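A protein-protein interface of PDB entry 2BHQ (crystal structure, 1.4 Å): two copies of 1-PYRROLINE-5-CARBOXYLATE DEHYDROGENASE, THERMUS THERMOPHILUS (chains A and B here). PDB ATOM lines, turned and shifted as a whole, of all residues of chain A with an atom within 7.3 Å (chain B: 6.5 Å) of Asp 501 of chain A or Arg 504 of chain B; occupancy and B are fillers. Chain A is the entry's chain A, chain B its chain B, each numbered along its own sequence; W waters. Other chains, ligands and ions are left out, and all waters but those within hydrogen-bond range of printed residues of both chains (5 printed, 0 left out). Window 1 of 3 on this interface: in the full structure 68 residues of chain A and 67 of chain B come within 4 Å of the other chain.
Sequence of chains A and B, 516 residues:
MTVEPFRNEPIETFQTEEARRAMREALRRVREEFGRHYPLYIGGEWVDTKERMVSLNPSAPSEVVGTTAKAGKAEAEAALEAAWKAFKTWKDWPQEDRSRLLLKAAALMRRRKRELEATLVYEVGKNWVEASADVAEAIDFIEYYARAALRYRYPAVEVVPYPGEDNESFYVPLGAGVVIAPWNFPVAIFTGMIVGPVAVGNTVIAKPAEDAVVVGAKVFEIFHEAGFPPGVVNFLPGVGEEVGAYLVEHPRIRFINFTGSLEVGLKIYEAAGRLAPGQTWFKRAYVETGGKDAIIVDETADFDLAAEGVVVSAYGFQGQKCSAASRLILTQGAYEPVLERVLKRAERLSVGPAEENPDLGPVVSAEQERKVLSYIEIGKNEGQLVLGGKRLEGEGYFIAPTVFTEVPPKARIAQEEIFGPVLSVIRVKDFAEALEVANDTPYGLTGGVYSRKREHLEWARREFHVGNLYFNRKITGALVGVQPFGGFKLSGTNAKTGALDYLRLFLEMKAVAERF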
ATOM      1  N   TYR A 144      18.063   4.649 -13.540  1.00  0.00           N
ATOM      2  CA  TYR A 144      16.716   4.854 -13.022  1.00  0.00           C
ATOM      3  C   TYR A 144      16.644   4.723 -11.503  1.00  0.00           C
ATOM      4  O   TYR A 144      16.119   5.609 -10.822  1.00  0.00           O
ATOM      5  CB  TYR A 144      15.748   3.857 -13.667  1.00  0.00           C
ATOM      6  CG  TYR A 144      14.299   4.122 -13.321  1.00  0.00           C
ATOM      7  CD1 TYR A 144      13.522   4.983 -14.093  1.00  0.00           C
ATOM      8  CD2 TYR A 144      13.721   3.541 -12.196  1.00  0.00           C
ATOM      9  CE1 TYR A 144      12.192   5.260 -13.747  1.00  0.00           C
ATOM     10  CE2 TYR A 144      12.404   3.811 -11.841  1.00  0.00           C
ATOM     11  CZ  TYR A 144      11.645   4.670 -12.618  1.00  0.00           C
ATOM     12  OH  TYR A 144      10.339   4.939 -12.262  1.00  0.00           O
ATOM     13  N   TYR A 145      17.163   3.622 -10.967  1.00  0.00           N
ATOM     14  CA  TYR A 145      17.109   3.417  -9.522  1.00  0.00           C
ATOM     15  C   TYR A 145      17.933   4.453  -8.752  1.00  0.00           C
ATOM     16  O   TYR A 145      17.590   4.797  -7.619  1.00  0.00           O
ATOM     17  CB  TYR A 145      17.555   1.993  -9.158  1.00  0.00           C
ATOM     18  CG  TYR A 145      16.614   0.899  -9.639  1.00  0.00           C
ATOM     19  CD1 TYR A 145      17.095  -0.378  -9.921  1.00  0.00           C
ATOM     20  CD2 TYR A 145      15.249   1.144  -9.824  1.00  0.00           C
ATOM     21  CE1 TYR A 145      16.252  -1.386 -10.383  1.00  0.00           C
ATOM     22  CE2 TYR A 145      14.387   0.139 -10.288  1.00  0.00           C
ATOM     23  CZ  TYR A 145      14.898  -1.121 -10.568  1.00  0.00           C
ATOM     24  OH  TYR A 145      14.071  -2.104 -11.061  1.00  0.00           O
ATOM     25  N   ALA A 148      15.433   7.248  -8.639  1.00  0.00           N
ATOM     26  CA  ALA A 148      14.248   6.862  -7.878  1.00  0.00           C
ATOM     27  C   ALA A 148      14.510   6.794  -6.379  1.00  0.00           C
ATOM     28  O   ALA A 148      13.652   7.164  -5.574  1.00  0.00           O
ATOM     29  CB  ALA A 148      13.720   5.513  -8.384  1.00  0.00           C
ATOM     30  N   TYR A 152      12.865   8.651  -1.917  1.00  0.00           N
ATOM     31  CA  TYR A 152      12.584   8.051  -0.613  1.00  0.00           C
ATOM     32  C   TYR A 152      13.479   8.606   0.498  1.00  0.00           C
ATOM     33  O   TYR A 152      13.428   8.124   1.631  1.00  0.00           O
ATOM     34  CB  TYR A 152      12.781   6.529  -0.673  1.00  0.00           C
ATOM     35  CG  TYR A 152      11.804   5.792  -1.566  1.00  0.00           C
ATOM     36  CD1 TYR A 152      12.084   5.565  -2.915  1.00  0.00           C
ATOM     37  CD2 TYR A 152      10.589   5.334  -1.060  1.00  0.00           C
ATOM     38  CE1 TYR A 152      11.175   4.900  -3.738  1.00  0.00           C
ATOM     39  CE2 TYR A 152       9.674   4.669  -1.870  1.00  0.00           C
ATOM     40  CZ  TYR A 152       9.972   4.456  -3.206  1.00  0.00           C
ATOM     41  OH  TYR A 152       9.064   3.797  -4.004  1.00  0.00           O
ATOM     42  N   ASN A 494       4.321  -9.432  -8.554  1.00  0.00           N
ATOM     43  CA  ASN A 494       4.069  -8.100  -9.108  1.00  0.00           C
ATOM     44  C   ASN A 494       5.071  -7.045  -8.634  1.00  0.00           C
ATOM     45  O   ASN A 494       4.704  -5.894  -8.402  1.00  0.00           O
ATOM     46  CB  ASN A 494       2.633  -7.641  -8.784  1.00  0.00           C
ATOM     47  CG  ASN A 494       2.176  -6.469  -9.649  1.00  0.00           C
ATOM     48  OD1 ASN A 494       1.841  -5.398  -9.140  1.00  0.00           O
ATOM     49  ND2 ASN A 494       2.156  -6.674 -10.962  1.00  0.00           N
ATOM     50  N   ALA A 495       6.329  -7.438  -8.463  1.00  0.00           N
ATOM     51  CA  ALA A 495       7.352  -6.472  -8.075  1.00  0.00           C
ATOM     52  C   ALA A 495       7.692  -5.792  -9.393  1.00  0.00           C
ATOM     53  O   ALA A 495       8.404  -6.351 -10.224  1.00  0.00           O
ATOM     54  CB  ALA A 495       8.576  -7.180  -7.510  1.00  0.00           C
ATOM     55  N   LYS A 496       7.162  -4.593  -9.595  1.00  0.00           N
ATOM     56  CA  LYS A 496       7.383  -3.872 -10.844  1.00  0.00           C
ATOM     57  C   LYS A 496       8.777  -3.288 -11.005  1.00  0.00           C
ATOM     58  O   LYS A 496       9.102  -2.259 -10.417  1.00  0.00           O
ATOM     59  CB  LYS A 496       6.340  -2.764 -10.991  1.00  0.00           C
ATOM     60  CG  LYS A 496       4.935  -3.259 -11.332  1.00  0.00           C
ATOM     61  CD  LYS A 496       4.925  -3.970 -12.683  1.00  0.00           C
ATOM     62  CE  LYS A 496       3.600  -3.801 -13.406  1.00  0.00           C
ATOM     63  NZ  LYS A 496       3.620  -4.485 -14.731  1.00  0.00           N
ATOM     64  N   THR A 497       9.601  -3.935 -11.822  1.00  0.00           N
ATOM     65  CA  THR A 497      10.953  -3.439 -12.039  1.00  0.00           C
ATOM     66  C   THR A 497      10.922  -2.201 -12.927  1.00  0.00           C
ATOM     67  O   THR A 497       9.991  -2.006 -13.710  1.00  0.00           O
ATOM     68  CB  THR A 497      11.848  -4.507 -12.702  1.00  0.00           C
ATOM     69  OG1 THR A 497      11.370  -4.791 -14.024  1.00  0.00           O
ATOM     70  CG2 THR A 497      11.844  -5.789 -11.878  1.00  0.00           C
ATOM     71  N   GLY A 498      11.935  -1.351 -12.792  1.00  0.00           N
ATOM     72  CA  GLY A 498      11.988  -0.143 -13.597  1.00  0.00           C
ATOM     73  C   GLY A 498      10.877   0.834 -13.257  1.00  0.00           C
ATOM     74  O   GLY A 498      10.425   1.602 -14.112  1.00  0.00           O
ATOM     75  N   ALA A 499      10.436   0.799 -12.003  1.00  0.00           N
ATOM     76  CA  ALA A 499       9.375   1.674 -11.526  1.00  0.00           C
ATOM     77  C   ALA A 499       9.703   2.161 -10.119  1.00  0.00           C
ATOM     78  O   ALA A 499      10.405   1.488  -9.367  1.00  0.00           O
ATOM     79  CB  ALA A 499       8.051   0.927 -11.518  1.00  0.00           C
ATOM     80  N   LEU A 500       9.181   3.329  -9.772  1.00  0.00           N
ATOM     81  CA  LEU A 500       9.410   3.908  -8.456  1.00  0.00           C
ATOM     82  C   LEU A 500       9.035   2.933  -7.335  1.00  0.00           C
ATOM     83  O   LEU A 500       9.745   2.834  -6.333  1.00  0.00           O
ATOM     84  CB  LEU A 500       8.588   5.190  -8.309  1.00  0.00           C
ATOM     85  CG  LEU A 500       8.935   6.336  -9.264  1.00  0.00           C
ATOM     86  CD1 LEU A 500       7.893   7.441  -9.166  1.00  0.00           C
ATOM     87  CD2 LEU A 500      10.315   6.864  -8.933  1.00  0.00           C
ATOM     88  N   ASP A 501       7.929   2.214  -7.521  1.00  0.00           N
ATOM     89  CA  ASP A 501       7.431   1.266  -6.525  1.00  0.00           C
ATOM     90  C   ASP A 501       8.389   0.135  -6.186  1.00  0.00           C
ATOM     91  O   ASP A 501       8.322  -0.431  -5.097  1.00  0.00           O
ATOM     92  CB  ASP A 501       6.105   0.648  -6.990  1.00  0.00           C
ATOM     93  CG  ASP A 501       4.930   1.587  -6.835  1.00  0.00           C
ATOM     94  OD1 ASP A 501       5.127   2.750  -6.423  1.00  0.00           O
ATOM     95  OD2 ASP A 501       3.801   1.151  -7.135  1.00  0.00           O
ATOM     96  N   TYR A 502       9.280  -0.201  -7.112  1.00  0.00           N
ATOM     97  CA  TYR A 502      10.214  -1.294  -6.873  1.00  0.00           C
ATOM     98  C   TYR A 502      11.053  -1.103  -5.615  1.00  0.00           C
ATOM     99  O   TYR A 502      11.207  -2.026  -4.820  1.00  0.00           O
ATOM    100  CB  TYR A 502      11.149  -1.456  -8.072  1.00  0.00           C
ATOM    101  CG  TYR A 502      11.948  -2.740  -8.079  1.00  0.00           C
ATOM    102  CD1 TYR A 502      11.314  -3.974  -8.218  1.00  0.00           C
ATOM    103  CD2 TYR A 502      13.342  -2.719  -8.023  1.00  0.00           C
ATOM    104  CE1 TYR A 502      12.048  -5.157  -8.311  1.00  0.00           C
ATOM    105  CE2 TYR A 502      14.086  -3.894  -8.119  1.00  0.00           C
ATOM    106  CZ  TYR A 502      13.433  -5.105  -8.267  1.00  0.00           C
ATOM    107  OH  TYR A 502      14.169  -6.261  -8.411  1.00  0.00           O
ATOM    108  N   LEU A 503      11.585   0.099  -5.426  1.00  0.00           N
ATOM    109  CA  LEU A 503      12.447   0.361  -4.279  1.00  0.00           C
ATOM    110  C   LEU A 503      11.740   0.298  -2.927  1.00  0.00           C
ATOM    111  O   LEU A 503      12.363  -0.030  -1.913  1.00  0.00           O
ATOM    112  CB  LEU A 503      13.154   1.712  -4.456  1.00  0.00           C
ATOM    113  CG  LEU A 503      13.942   1.865  -5.770  1.00  0.00           C
ATOM    114  CD1 LEU A 503      14.718   3.180  -5.748  1.00  0.00           C
ATOM    115  CD2 LEU A 503      14.897   0.694  -5.963  1.00  0.00           C
ATOM    116  N   ARG A 504      10.444   0.599  -2.910  1.00  0.00           N
ATOM    117  CA  ARG A 504       9.675   0.559  -1.671  1.00  0.00           C
ATOM    118  C   ARG A 504       9.700  -0.845  -1.074  1.00  0.00           C
ATOM    119  O   ARG A 504       9.578  -1.023   0.140  1.00  0.00           O
ATOM    120  CB  ARG A 504       8.221   0.971  -1.943  1.00  0.00           C
ATOM    121  CG  ARG A 504       7.321   0.945  -0.710  1.00  0.00           C
ATOM    122  CD  ARG A 504       7.794   1.952   0.327  1.00  0.00           C
ATOM    123  NE  ARG A 504       6.981   1.936   1.542  1.00  0.00           N
ATOM    124  CZ  ARG A 504       7.132   1.073   2.543  1.00  0.00           C
ATOM    125  NH1 ARG A 504       6.337   1.153   3.606  1.00  0.00           N
ATOM    126  NH2 ARG A 504       8.076   0.142   2.496  1.00  0.00           N
ATOM    127  N   LEU A 505       9.854  -1.843  -1.939  1.00  0.00           N
ATOM    128  CA  LEU A 505       9.888  -3.235  -1.510  1.00  0.00           C
ATOM    129  C   LEU A 505      11.082  -3.561  -0.625  1.00  0.00           C
ATOM    130  O   LEU A 505      11.056  -4.538   0.123  1.00  0.00           O
ATOM    131  CB  LEU A 505       9.924  -4.155  -2.730  1.00  0.00           C
ATOM    132  CG  LEU A 505       8.732  -4.066  -3.683  1.00  0.00           C
ATOM    133  CD1 LEU A 505       9.021  -4.904  -4.918  1.00  0.00           C
ATOM    134  CD2 LEU A 505       7.466  -4.532  -2.987  1.00  0.00           C
ATOM    135  N   PHE A 506      12.129  -2.743  -0.698  1.00  0.00           N
ATOM    136  CA  PHE A 506      13.341  -3.007   0.073  1.00  0.00           C
ATOM    137  C   PHE A 506      13.555  -2.015   1.208  1.00  0.00           C
ATOM    138  O   PHE A 506      14.682  -1.787   1.665  1.00  0.00           O
ATOM    139  CB  PHE A 506      14.553  -2.955  -0.862  1.00  0.00           C
ATOM    140  CG  PHE A 506      14.301  -3.560  -2.213  1.00  0.00           C
ATOM    141  CD1 PHE A 506      14.490  -2.807  -3.371  1.00  0.00           C
ATOM    142  CD2 PHE A 506      13.867  -4.877  -2.333  1.00  0.00           C
ATOM    143  CE1 PHE A 506      14.248  -3.357  -4.629  1.00  0.00           C
ATOM    144  CE2 PHE A 506      13.622  -5.436  -3.588  1.00  0.00           C
ATOM    145  CZ  PHE A 506      13.813  -4.672  -4.738  1.00  0.00           C
ATOM    146  N   TYR B 152      -4.560   6.950  -5.270  1.00  0.00           N
ATOM    147  CA  TYR B 152      -4.207   5.837  -6.148  1.00  0.00           C
ATOM    148  C   TYR B 152      -5.134   5.706  -7.356  1.00  0.00           C
ATOM    149  O   TYR B 152      -5.020   4.745  -8.122  1.00  0.00           O
ATOM    150  CB  TYR B 152      -4.249   4.515  -5.368  1.00  0.00           C
ATOM    151  CG  TYR B 152      -3.239   4.397  -4.253  1.00  0.00           C
ATOM    152  CD1 TYR B 152      -3.542   4.803  -2.954  1.00  0.00           C
ATOM    153  CD2 TYR B 152      -1.970   3.885  -4.500  1.00  0.00           C
ATOM    154  CE1 TYR B 152      -2.601   4.699  -1.926  1.00  0.00           C
ATOM    155  CE2 TYR B 152      -1.024   3.778  -3.484  1.00  0.00           C
ATOM    156  CZ  TYR B 152      -1.348   4.185  -2.199  1.00  0.00           C
ATOM    157  OH  TYR B 152      -0.416   4.066  -1.193  1.00  0.00           O
ATOM    158  N   VAL B 157       0.156   5.989 -11.748  1.00  0.00           N
ATOM    159  CA  VAL B 157       1.597   5.779 -11.812  1.00  0.00           C
ATOM    160  C   VAL B 157       2.390   6.728 -12.698  1.00  0.00           C
ATOM    161  O   VAL B 157       2.040   6.969 -13.849  1.00  0.00           O
ATOM    162  CB  VAL B 157       1.903   4.332 -12.224  1.00  0.00           C
ATOM    163  CG1 VAL B 157       3.400   4.069 -12.145  1.00  0.00           C
ATOM    164  CG2 VAL B 157       1.148   3.369 -11.310  1.00  0.00           C
ATOM    165  N   TYR B 171      -3.257   1.193 -10.926  1.00  0.00           N
ATOM    166  CA  TYR B 171      -3.475   0.179  -9.909  1.00  0.00           C
ATOM    167  C   TYR B 171      -4.856  -0.448  -9.979  1.00  0.00           C
ATOM    168  O   TYR B 171      -5.826   0.183 -10.408  1.00  0.00           O
ATOM    169  CB  TYR B 171      -3.286   0.778  -8.513  1.00  0.00           C
ATOM    170  CG  TYR B 171      -1.904   1.317  -8.267  1.00  0.00           C
ATOM    171  CD1 TYR B 171      -1.679   2.689  -8.161  1.00  0.00           C
ATOM    172  CD2 TYR B 171      -0.817   0.458  -8.149  1.00  0.00           C
ATOM    173  CE1 TYR B 171      -0.403   3.191  -7.943  1.00  0.00           C
ATOM    174  CE2 TYR B 171       0.468   0.950  -7.934  1.00  0.00           C
ATOM    175  CZ  TYR B 171       0.663   2.319  -7.832  1.00  0.00           C
ATOM    176  OH  TYR B 171       1.923   2.825  -7.619  1.00  0.00           O
ATOM    177  N   VAL B 200     -10.178   0.493  -1.811  1.00  0.00           N
ATOM    178  CA  VAL B 200      -9.575   0.472  -3.137  1.00  0.00           C
ATOM    179  C   VAL B 200     -10.095  -0.600  -4.096  1.00  0.00           C
ATOM    180  O   VAL B 200      -9.507  -0.832  -5.154  1.00  0.00           O
ATOM    181  CB  VAL B 200      -8.024   0.387  -3.054  1.00  0.00           C
ATOM    182  CG1 VAL B 200      -7.477   1.635  -2.358  1.00  0.00           C
ATOM    183  CG2 VAL B 200      -7.594  -0.872  -2.311  1.00  0.00           C
ATOM    184  N   ARG B 284      -0.776 -12.799  -0.469  1.00  0.00           N
ATOM    185  CA  ARG B 284      -0.160 -11.723   0.286  1.00  0.00           C
ATOM    186  C   ARG B 284      -0.728 -11.864   1.686  1.00  0.00           C
ATOM    187  O   ARG B 284      -1.936 -12.055   1.857  1.00  0.00           O
ATOM    188  CB  ARG B 284      -0.529 -10.345  -0.274  1.00  0.00           C
ATOM    189  CG  ARG B 284       0.044 -10.058  -1.644  1.00  0.00           C
ATOM    190  CD  ARG B 284      -0.103  -8.589  -1.989  1.00  0.00           C
ATOM    191  NE  ARG B 284       0.340  -8.322  -3.352  1.00  0.00           N
ATOM    192  CZ  ARG B 284       0.291  -7.131  -3.938  1.00  0.00           C
ATOM    193  NH1 ARG B 284      -0.186  -6.077  -3.286  1.00  0.00           N
ATOM    194  NH2 ARG B 284       0.721  -6.998  -5.183  1.00  0.00           N
ATOM    195  N   TYR B 286      -0.486  -9.981   5.501  1.00  0.00           N
ATOM    196  CA  TYR B 286      -0.011  -8.869   6.304  1.00  0.00           C
ATOM    197  C   TYR B 286      -0.314  -9.210   7.747  1.00  0.00           C
ATOM    198  O   TYR B 286      -1.454  -9.515   8.092  1.00  0.00           O
ATOM    199  CB  TYR B 286      -0.704  -7.581   5.877  1.00  0.00           C
ATOM    200  CG  TYR B 286      -0.441  -7.292   4.426  1.00  0.00           C
ATOM    201  CD1 TYR B 286      -1.443  -7.439   3.473  1.00  0.00           C
ATOM    202  CD2 TYR B 286       0.839  -6.949   3.991  1.00  0.00           C
ATOM    203  CE1 TYR B 286      -1.178  -7.258   2.119  1.00  0.00           C
ATOM    204  CE2 TYR B 286       1.115  -6.765   2.643  1.00  0.00           C
ATOM    205  CZ  TYR B 286       0.104  -6.921   1.713  1.00  0.00           C
ATOM    206  OH  TYR B 286       0.375  -6.734   0.380  1.00  0.00           O
ATOM    207  N   LEU B 500      -0.603   6.418   4.094  1.00  0.00           N
ATOM    208  CA  LEU B 500      -0.862   6.268   2.667  1.00  0.00           C
ATOM    209  C   LEU B 500      -0.378   4.913   2.152  1.00  0.00           C
ATOM    210  O   LEU B 500      -1.050   4.262   1.345  1.00  0.00           O
ATOM    211  CB  LEU B 500      -0.160   7.388   1.897  1.00  0.00           C
ATOM    212  CG  LEU B 500      -0.612   8.810   2.241  1.00  0.00           C
ATOM    213  CD1 LEU B 500       0.293   9.817   1.551  1.00  0.00           C
ATOM    214  CD2 LEU B 500      -2.058   9.010   1.816  1.00  0.00           C
ATOM    215  N   ASP B 501       0.785   4.487   2.636  1.00  0.00           N
ATOM    216  CA  ASP B 501       1.391   3.222   2.219  1.00  0.00           C
ATOM    217  C   ASP B 501       0.548   1.977   2.489  1.00  0.00           C
ATOM    218  O   ASP B 501       0.704   0.962   1.813  1.00  0.00           O
ATOM    219  CB  ASP B 501       2.752   3.034   2.902  1.00  0.00           C
ATOM    220  CG  ASP B 501       3.859   3.858   2.264  1.00  0.00           C
ATOM    221  OD1 ASP B 501       3.580   4.681   1.362  1.00  0.00           O
ATOM    222  OD2 ASP B 501       5.025   3.679   2.679  1.00  0.00           O
ATOM    223  N   TYR B 502      -0.346   2.046   3.466  1.00  0.00           N
ATOM    224  CA  TYR B 502      -1.158   0.881   3.798  1.00  0.00           C
ATOM    225  C   TYR B 502      -1.981   0.373   2.622  1.00  0.00           C
ATOM    226  O   TYR B 502      -2.041  -0.827   2.381  1.00  0.00           O
ATOM    227  CB  TYR B 502      -2.095   1.215   4.960  1.00  0.00           C
ATOM    228  CG  TYR B 502      -2.776   0.022   5.594  1.00  0.00           C
ATOM    229  CD1 TYR B 502      -2.041  -0.930   6.303  1.00  0.00           C
ATOM    230  CD2 TYR B 502      -4.163  -0.103   5.567  1.00  0.00           C
ATOM    231  CE1 TYR B 502      -2.676  -1.968   6.987  1.00  0.00           C
ATOM    232  CE2 TYR B 502      -4.810  -1.138   6.243  1.00  0.00           C
ATOM    233  CZ  TYR B 502      -4.060  -2.058   6.955  1.00  0.00           C
ATOM    234  OH  TYR B 502      -4.708  -3.034   7.679  1.00  0.00           O
ATOM    235  N   LEU B 503      -2.604   1.288   1.886  1.00  0.00           N
ATOM    236  CA  LEU B 503      -3.467   0.891   0.782  1.00  0.00           C
ATOM    237  C   LEU B 503      -2.747   0.235  -0.391  1.00  0.00           C
ATOM    238  O   LEU B 503      -3.333  -0.584  -1.099  1.00  0.00           O
ATOM    239  CB  LEU B 503      -4.286   2.094   0.306  1.00  0.00           C
ATOM    240  CG  LEU B 503      -5.141   2.761   1.396  1.00  0.00           C
ATOM    241  CD1 LEU B 503      -6.014   3.842   0.758  1.00  0.00           C
ATOM    242  CD2 LEU B 503      -6.016   1.725   2.103  1.00  0.00           C
ATOM    243  N   ARG B 504      -1.477   0.581  -0.584  1.00  0.00           N
ATOM    244  CA  ARG B 504      -0.677   0.017  -1.669  1.00  0.00           C
ATOM    245  C   ARG B 504      -0.550  -1.501  -1.524  1.00  0.00           C
ATOM    246  O   ARG B 504      -0.388  -2.228  -2.510  1.00  0.00           O
ATOM    247  CB  ARG B 504       0.721   0.643  -1.668  1.00  0.00           C
ATOM    248  CG  ARG B 504       1.637   0.117  -2.766  1.00  0.00           C
ATOM    249  CD  ARG B 504       1.108   0.490  -4.142  1.00  0.00           C
ATOM    250  NE  ARG B 504       1.961  -0.007  -5.222  1.00  0.00           N
ATOM    251  CZ  ARG B 504       1.977  -1.263  -5.660  1.00  0.00           C
ATOM    252  NH1 ARG B 504       2.792  -1.599  -6.655  1.00  0.00           N
ATOM    253  NH2 ARG B 504       1.179  -2.177  -5.119  1.00  0.00           N
ATOM    254  N   LEU B 505      -0.612  -1.971  -0.285  1.00  0.00           N
ATOM    255  CA  LEU B 505      -0.500  -3.395   0.003  1.00  0.00           C
ATOM    256  C   LEU B 505      -1.647  -4.200  -0.591  1.00  0.00           C
ATOM    257  O   LEU B 505      -1.522  -5.405  -0.802  1.00  0.00           O
ATOM    258  CB  LEU B 505      -0.473  -3.622   1.516  1.00  0.00           C
ATOM    259  CG  LEU B 505       0.673  -2.964   2.286  1.00  0.00           C
ATOM    260  CD1 LEU B 505       0.446  -3.137   3.782  1.00  0.00           C
ATOM    261  CD2 LEU B 505       1.991  -3.581   1.860  1.00  0.00           C
ATOM    262  N   PHE B 506      -2.763  -3.533  -0.871  1.00  0.00           N
ATOM    263  CA  PHE B 506      -3.942  -4.216  -1.394  1.00  0.00           C
ATOM    264  C   PHE B 506      -4.205  -3.911  -2.862  1.00  0.00           C
ATOM    265  O   PHE B 506      -5.332  -4.033  -3.352  1.00  0.00           O
ATOM    266  CB  PHE B 506      -5.174  -3.805  -0.577  1.00  0.00           C
ATOM    267  CG  PHE B 506      -4.907  -3.657   0.898  1.00  0.00           C
ATOM    268  CD1 PHE B 506      -5.242  -2.479   1.561  1.00  0.00           C
ATOM    269  CD2 PHE B 506      -4.312  -4.685   1.620  1.00  0.00           C
ATOM    270  CE1 PHE B 506      -4.988  -2.325   2.921  1.00  0.00           C
ATOM    271  CE2 PHE B 506      -4.052  -4.543   2.984  1.00  0.00           C
ATOM    272  CZ  PHE B 506      -4.392  -3.359   3.636  1.00  0.00           C
ATOM    273  N   LEU B 507      -3.141  -3.541  -3.566  1.00  0.00           N
ATOM    274  CA  LEU B 507      -3.222  -3.217  -4.984  1.00  0.00           C
ATOM    275  C   LEU B 507      -2.084  -3.866  -5.756  1.00  0.00           C
ATOM    276  O   LEU B 507      -1.046  -4.184  -5.183  1.00  0.00           O
ATOM    277  CB  LEU B 507      -3.116  -1.701  -5.188  1.00  0.00           C
ATOM    278  CG  LEU B 507      -4.211  -0.806  -4.613  1.00  0.00           C
ATOM    279  CD1 LEU B 507      -3.744   0.643  -4.646  1.00  0.00           C
ATOM    280  CD2 LEU B 507      -5.502  -0.989  -5.402  1.00  0.00           C
ATOM    281  N   GLU B 508      -2.302  -4.082  -7.049  1.00  0.00           N
ATOM    282  CA  GLU B 508      -1.262  -4.585  -7.936  1.00  0.00           C
ATOM    283  C   GLU B 508      -1.271  -3.609  -9.118  1.00  0.00           C
ATOM    284  O   GLU B 508      -2.248  -2.879  -9.318  1.00  0.00           O
ATOM    285  CB  GLU B 508      -1.505  -6.045  -8.362  1.00  0.00           C
ATOM    286  CG  GLU B 508      -2.857  -6.397  -8.936  1.00  0.00           C
ATOM    287  CD  GLU B 508      -3.042  -7.911  -9.045  1.00  0.00           C
ATOM    288  OE1 GLU B 508      -2.076  -8.658  -8.757  1.00  0.00           O
ATOM    289  OE2 GLU B 508      -4.147  -8.358  -9.409  1.00  0.00           O
ATOM    290  N   MET B 509      -0.180  -3.561  -9.873  1.00  0.00           N
ATOM    291  CA  MET B 509      -0.064  -2.617 -10.983  1.00  0.00           C
ATOM    292  C   MET B 509      -0.074  -3.239 -12.368  1.00  0.00           C
ATOM    293  O   MET B 509       0.502  -4.310 -12.589  1.00  0.00           O
ATOM    294  CB  MET B 509       1.229  -1.806 -10.829  1.00  0.00           C
ATOM    295  CG  MET B 509       1.333  -0.584 -11.749  1.00  0.00           C
ATOM    296  SD  MET B 509       3.037   0.017 -11.964  1.00  0.00           S
ATOM    297  CE  MET B 509       3.460   0.507 -10.285  1.00  0.00           C
HETATM  298  O   HOH W   1       2.723   3.437  -4.471  1.00  0.00           O
HETATM  299  O   HOH W   2       2.071  -4.647  -6.539  1.00  0.00           O
HETATM  300  O   HOH W   3       5.252  -3.210  -7.739  1.00  0.00           O
HETATM  301  O   HOH W   4       3.419  -0.520   2.763  1.00  0.00           O
HETATM  302  O   HOH W   5       3.973   4.632  -8.253  1.00  0.00           O
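Among the printed residues, merely in contact across the chains: Asn 494 of chain A with Glu 508 of chain B (3.4 Å), Lys 496 of chain A with Met 509 of chain B (3.2 Å) and Asp 501 of chain A with Met 509 of chain B (3.2 Å).
Asp 501 of chain A touches Arg 504 of chain B, and with the chains exchanged Arg 504 of chain A touches Asp 501 of chain B. Positions printed for both chains: 152, 500, 501, 502, 503, 504, 505 and 506.
The guanidinium group (NH2) of Arg 504 of chain B lies within hydrogen-bond range of the backbone carbonyl oxygen (O) of Leu 507 of chain B, at 3.0 Å.
Water W5 lies within hydrogen-bond range of OH of Tyr 171 of chain B and OD1 of Asp 501 of chain A. Water W1 bridges the side-chain carboxylate (OD1) of Asp 501 of chain A (3.2 Å) and the side-chain hydroxyl (OH) of Tyr 171 of chain B (3.3 Å). Water W4 bridges O of Asp 501 of chain B and NH1 of Arg 504 of chain A.
The side-chain amide oxygen of Asn 494 of chain A is in hydrogen-bond range of the backbone NH of Met 509 of chain B, at 2.8 Å. The guanidinium group (NE) of Arg 504 of chain A is in salt-bridge range of the side-chain carboxylate (OD2) of Asp 501 of chain B, at 2.9 Å. The side-chain carboxylate of Asp 501 of chain A is in hydrogen-bond range of the side-chain hydroxyl of Tyr 171 of chain B (2.6 Å). The guanidinium group of Arg 504 of chain B lies within salt-bridge range of the side-chain carboxylate of Asp 501 of chain A, 2.9 Å away.
Asp 501 of chain A touches just these residues of chain B: Tyr 171, Arg 504 and Met 509. Of chain A, only Asp 501 comes within 4 Å of Arg 504 of chain B. Of the printed residues of chain A, Asp 501 of chain B touches Arg 504 (2.9 Å). Of the printed residues of chain A, Glu 508 of chain B touches Asn 494 (3.4 Å). Of the printed residues of chain A, Tyr 171 of chain B touches Asp 501. Of the printed residues of chain A, Met 509 of chain B touches Asn 494, Lys 496 and Asp 501. Of the printed residues of chain B, Arg 504 of chain A touches Asp 501. The nearest residue of chain A that does not touch Arg 504 of chain B is Asn 494 of chain A (4.6 Å).
Printed residues of chain A that touch a printed residue of chain B: Asn 494, Lys 496, Asp 501 and Arg 504. Among the printed residues, 7 pairs touch across the chains. Among the printed residues, Asp or Glu carboxylates within 4 Å of a Lys or Arg side-chain nitrogen of the other chain: Asp 501 of chain A with Arg 504 of chain B (2.9 Å) and Arg 504 of chain A with Asp 501 of chain B (2.9 Å).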
